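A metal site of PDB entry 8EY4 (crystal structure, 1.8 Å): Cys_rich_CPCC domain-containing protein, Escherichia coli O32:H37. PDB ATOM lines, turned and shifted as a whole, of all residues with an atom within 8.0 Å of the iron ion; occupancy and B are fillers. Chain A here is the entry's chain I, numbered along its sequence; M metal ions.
The iron ion is bound by the side-chain sulfur of Cys 29 (2.3 Å), the side-chain sulfur of Cys 12 (2.3 Å), the side-chain sulfur of Cys 26 (2.3 Å) and the side-chain sulfur of Cys 9 (2.4 Å).
SG of Cys 26 lies close to OG1 of Thr 16, at 3.3 Å. The side-chain sulfur (SG) of Cys 29 lies close to the backbone NH (N) of Trp 31 (3.6 Å). N of Cys 11 sits close to SG of Cys 9, 3.4 Å away. N of Cys 26 sits at hydrogen-bond distance from O of Trp 31. The side-chain amide nitrogen (ND2) of Asn 14 sits close to the side-chain sulfur (SG) of Cys 12 (3.4 Å). The backbone carbonyl oxygen (O) of Asn 14 lies within hydrogen-bond range of the backbone NH (N) of Cys 9. The backbone NH of Ile 28 lies close to the side-chain sulfur of Cys 26, at 3.4 Å.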
ATOM      1  N   PRO A   8      26.019  -0.636   1.022  1.00  0.00           N
ATOM      2  CA  PRO A   8      25.191  -1.196   2.106  1.00  0.00           C
ATOM      3  C   PRO A   8      26.017  -1.811   3.226  1.00  0.00           C
ATOM      4  O   PRO A   8      26.993  -2.520   2.970  1.00  0.00           O
ATOM      5  CB  PRO A   8      24.354  -2.261   1.393  1.00  0.00           C
ATOM      6  CG  PRO A   8      25.176  -2.668   0.211  1.00  0.00           C
ATOM      7  CD  PRO A   8      25.879  -1.411  -0.229  1.00  0.00           C
ATOM      8  N   CYS A   9      25.619  -1.520   4.459  1.00  0.00           N
ATOM      9  CA  CYS A   9      26.133  -2.248   5.600  1.00  0.00           C
ATOM     10  C   CYS A   9      25.740  -3.724   5.437  1.00  0.00           C
ATOM     11  O   CYS A   9      24.572  -4.025   5.128  1.00  0.00           O
ATOM     12  CB  CYS A   9      25.580  -1.694   6.920  1.00  0.00           C
ATOM     13  SG  CYS A   9      25.959  -2.671   8.402  1.00  0.00           S
ATOM     14  N   PRO A  10      26.661  -4.649   5.609  1.00  0.00           N
ATOM     15  CA  PRO A  10      26.306  -6.073   5.452  1.00  0.00           C
ATOM     16  C   PRO A  10      25.332  -6.573   6.506  1.00  0.00           C
ATOM     17  O   PRO A  10      24.690  -7.613   6.291  1.00  0.00           O
ATOM     18  CB  PRO A  10      27.653  -6.802   5.547  1.00  0.00           C
ATOM     19  CG  PRO A  10      28.630  -5.834   6.055  1.00  0.00           C
ATOM     20  CD  PRO A  10      28.108  -4.427   5.845  1.00  0.00           C
ATOM     21  N   CYS A  11      25.186  -5.867   7.624  1.00  0.00           N
ATOM     22  CA  CYS A  11      24.249  -6.292   8.676  1.00  0.00           C
ATOM     23  C   CYS A  11      22.869  -5.700   8.411  1.00  0.00           C
ATOM     24  O   CYS A  11      21.921  -6.421   8.064  1.00  0.00           O
ATOM     25  CB  CYS A  11      24.765  -5.888  10.049  1.00  0.00           C
ATOM     26  SG  CYS A  11      23.680  -6.346  11.444  1.00  0.00           S
ATOM     27  N   CYS A  12      22.741  -4.389   8.579  1.00  0.00           N
ATOM     28  CA  CYS A  12      21.419  -3.782   8.475  1.00  0.00           C
ATOM     29  C   CYS A  12      20.999  -3.470   7.036  1.00  0.00           C
ATOM     30  O   CYS A  12      19.804  -3.204   6.799  1.00  0.00           O
ATOM     31  CB  CYS A  12      21.390  -2.509   9.338  1.00  0.00           C
ATOM     32  SG  CYS A  12      22.406  -1.124   8.796  1.00  0.00           S
ATOM     33  N   GLY A  13      21.910  -3.478   6.070  1.00  0.00           N
ATOM     34  CA  GLY A  13      21.567  -3.229   4.675  1.00  0.00           C
ATOM     35  C   GLY A  13      21.390  -1.773   4.287  1.00  0.00           C
ATOM     36  O   GLY A  13      21.245  -1.484   3.092  1.00  0.00           O
ATOM     37  N   ASN A  14      21.444  -0.839   5.234  1.00  0.00           N
ATOM     38  CA  ASN A  14      21.412   0.582   4.920  1.00  0.00           C
ATOM     39  C   ASN A  14      22.748   1.074   4.382  1.00  0.00           C
ATOM     40  O   ASN A  14      23.826   0.582   4.760  1.00  0.00           O
ATOM     41  CB  ASN A  14      21.022   1.378   6.164  1.00  0.00           C
ATOM     42  CG  ASN A  14      19.680   0.962   6.700  1.00  0.00           C
ATOM     43  OD1 ASN A  14      18.706   1.012   5.983  1.00  0.00           O
ATOM     44  ND2 ASN A  14      19.624   0.554   7.945  1.00  0.00           N
ATOM     45  N   LYS A  15      22.673   2.085   3.509  1.00  0.00           N
ATOM     46  CA  LYS A  15      23.833   2.596   2.762  1.00  0.00           C
ATOM     47  C   LYS A  15      24.640   3.528   3.660  1.00  0.00           C
ATOM     48  O   LYS A  15      24.482   4.750   3.622  1.00  0.00           O
ATOM     49  CB  LYS A  15      23.397   3.307   1.482  1.00  0.00           C
ATOM     50  CG  LYS A  15      23.379   2.420   0.239  1.00  0.00           C
ATOM     51  CD  LYS A  15      23.049   3.233  -1.023  1.00  0.00           C
ATOM     52  CE  LYS A  15      21.767   4.054  -0.873  1.00  0.00           C
ATOM     53  NZ  LYS A  15      21.359   4.820  -2.098  1.00  0.00           N
ATOM     54  N   THR A  16      25.558   2.949   4.454  1.00  0.00           N
ATOM     55  CA  THR A  16      26.347   3.729   5.391  1.00  0.00           C
ATOM     56  C   THR A  16      27.852   3.555   5.229  1.00  0.00           C
ATOM     57  O   THR A  16      28.595   4.151   5.987  1.00  0.00           O
ATOM     58  CB  THR A  16      26.011   3.346   6.828  1.00  0.00           C
ATOM     59  OG1 THR A  16      26.257   1.947   6.980  1.00  0.00           O
ATOM     60  CG2 THR A  16      24.547   3.669   7.194  1.00  0.00           C
ATOM     61  N   ILE A  17      28.298   2.711   4.305  1.00  0.00           N
ATOM     62  CA  ILE A  17      29.691   2.298   4.232  1.00  0.00           C
ATOM     63  C   ILE A  17      30.359   3.054   3.100  1.00  0.00           C
ATOM     64  O   ILE A  17      29.777   3.206   2.017  1.00  0.00           O
ATOM     65  CB  ILE A  17      29.797   0.776   4.033  1.00  0.00           C
ATOM     66  CG1 ILE A  17      29.259   0.025   5.271  1.00  0.00           C
ATOM     67  CG2 ILE A  17      31.249   0.361   3.778  1.00  0.00           C
ATOM     68  CD1 ILE A  17      29.854   0.550   6.616  1.00  0.00           C
ATOM     69  N   ILE A  25      32.675   1.141  11.105  1.00  0.00           N
ATOM     70  CA  ILE A  25      31.621   0.774  12.041  1.00  0.00           C
ATOM     71  C   ILE A  25      30.334   1.476  11.614  1.00  0.00           C
ATOM     72  O   ILE A  25      30.285   2.698  11.521  1.00  0.00           O
ATOM     73  CB  ILE A  25      31.984   1.093  13.489  1.00  0.00           C
ATOM     74  CG1 ILE A  25      33.255   0.303  13.901  1.00  0.00           C
ATOM     75  CG2 ILE A  25      30.833   0.779  14.407  1.00  0.00           C
ATOM     76  CD1 ILE A  25      33.781   0.712  15.287  1.00  0.00           C
ATOM     77  N   CYS A  26      29.321   0.673  11.294  1.00  0.00           N
ATOM     78  CA  CYS A  26      28.035   1.217  10.859  1.00  0.00           C
ATOM     79  C   CYS A  26      27.440   2.058  11.974  1.00  0.00           C
ATOM     80  O   CYS A  26      27.278   1.546  13.096  1.00  0.00           O
ATOM     81  CB  CYS A  26      27.079   0.078  10.491  1.00  0.00           C
ATOM     82  SG  CYS A  26      25.454   0.724   9.942  1.00  0.00           S
ATOM     83  N   PRO A  27      27.084   3.320  11.715  1.00  0.00           N
ATOM     84  CA  PRO A  27      26.467   4.140  12.749  1.00  0.00           C
ATOM     85  C   PRO A  27      25.034   3.756  13.100  1.00  0.00           C
ATOM     86  O   PRO A  27      24.513   4.268  14.100  1.00  0.00           O
ATOM     87  CB  PRO A  27      26.493   5.548  12.137  1.00  0.00           C
ATOM     88  CG  PRO A  27      26.479   5.321  10.662  1.00  0.00           C
ATOM     89  CD  PRO A  27      27.280   4.030  10.448  1.00  0.00           C
ATOM     90  N   ILE A  28      24.368   2.945  12.294  1.00  0.00           N
ATOM     91  CA  ILE A  28      22.996   2.544  12.585  1.00  0.00           C
ATOM     92  C   ILE A  28      22.950   1.319  13.485  1.00  0.00           C
ATOM     93  O   ILE A  28      22.229   1.307  14.485  1.00  0.00           O
ATOM     94  CB  ILE A  28      22.221   2.309  11.282  1.00  0.00           C
ATOM     95  CG1 ILE A  28      22.090   3.627  10.505  1.00  0.00           C
ATOM     96  CG2 ILE A  28      20.827   1.690  11.583  1.00  0.00           C
ATOM     97  CD1 ILE A  28      21.517   3.463   9.074  1.00  0.00           C
ATOM     98  N   CYS A  29      23.709   0.276  13.155  1.00  0.00           N
ATOM     99  CA  CYS A  29      23.555  -0.999  13.824  1.00  0.00           C
ATOM    100  C   CYS A  29      24.801  -1.425  14.584  1.00  0.00           C
ATOM    101  O   CYS A  29      24.738  -2.413  15.332  1.00  0.00           O
ATOM    102  CB  CYS A  29      23.187  -2.079  12.801  1.00  0.00           C
ATOM    103  SG  CYS A  29      24.557  -2.561  11.655  1.00  0.00           S
ATOM    104  N   GLY A  30      25.914  -0.702  14.454  1.00  0.00           N
ATOM    105  CA  GLY A  30      27.114  -1.017  15.206  1.00  0.00           C
ATOM    106  C   GLY A  30      28.004  -2.091  14.615  1.00  0.00           C
ATOM    107  O   GLY A  30      29.080  -2.375  15.183  1.00  0.00           O
ATOM    108  N   TRP A  31      27.615  -2.690  13.499  1.00  0.00           N
ATOM    109  CA  TRP A  31      28.415  -3.755  12.887  1.00  0.00           C
ATOM    110  C   TRP A  31      29.701  -3.186  12.304  1.00  0.00           C
ATOM    111  O   TRP A  31      29.651  -2.240  11.512  1.00  0.00           O
ATOM    112  CB  TRP A  31      27.603  -4.429  11.770  1.00  0.00           C
ATOM    113  CG  TRP A  31      28.385  -5.535  11.075  1.00  0.00           C
ATOM    114  CD1 TRP A  31      28.962  -5.488   9.846  1.00  0.00           C
ATOM    115  CD2 TRP A  31      28.628  -6.845  11.591  1.00  0.00           C
ATOM    116  NE1 TRP A  31      29.568  -6.705   9.550  1.00  0.00           N
ATOM    117  CE2 TRP A  31      29.380  -7.548  10.615  1.00  0.00           C
ATOM    118  CE3 TRP A  31      28.292  -7.509  12.776  1.00  0.00           C
ATOM    119  CZ2 TRP A  31      29.816  -8.873  10.804  1.00  0.00           C
ATOM    120  CZ3 TRP A  31      28.719  -8.830  12.962  1.00  0.00           C
ATOM    121  CH2 TRP A  31      29.457  -9.485  11.979  1.00  0.00           C
ATOM    122  N   GLU A  32      30.865  -3.752  12.715  1.00  0.00           N
ATOM    123  CA  GLU A  32      32.132  -3.384  12.102  1.00  0.00           C
ATOM    124  C   GLU A  32      32.330  -4.192  10.829  1.00  0.00           C
ATOM    125  O   GLU A  32      32.171  -5.419  10.828  1.00  0.00           O
ATOM    126  CB  GLU A  32      33.302  -3.625  13.063  1.00  0.00           C
ATOM    127  CG  GLU A  32      34.609  -3.196  12.458  1.00  0.00           C
ATOM    128  CD  GLU A  32      35.726  -3.106  13.488  1.00  0.00           C
ATOM    129  OE1 GLU A  32      35.421  -3.300  14.675  1.00  0.00           O
ATOM    130  OE2 GLU A  32      36.881  -2.809  13.087  1.00  0.00           O
ATOM    131  N   PHE A  59      19.501  -7.447  15.086  1.00  0.00           N
ATOM    132  CA  PHE A  59      19.115  -6.123  14.609  1.00  0.00           C
ATOM    133  C   PHE A  59      17.693  -6.112  14.066  1.00  0.00           C
ATOM    134  O   PHE A  59      16.947  -5.142  14.265  1.00  0.00           O
ATOM    135  CB  PHE A  59      20.082  -5.619  13.543  1.00  0.00           C
ATOM    136  CG  PHE A  59      19.672  -4.292  12.978  1.00  0.00           C
ATOM    137  CD1 PHE A  59      19.948  -3.118  13.667  1.00  0.00           C
ATOM    138  CD2 PHE A  59      18.948  -4.213  11.787  1.00  0.00           C
ATOM    139  CE1 PHE A  59      19.539  -1.878  13.163  1.00  0.00           C
ATOM    140  CE2 PHE A  59      18.539  -2.973  11.284  1.00  0.00           C
ATOM    141  CZ  PHE A  59      18.836  -1.804  11.967  1.00  0.00           C
HETATM  142 FE    FE M   1      24.484  -1.383   9.713  1.00  0.00          FE
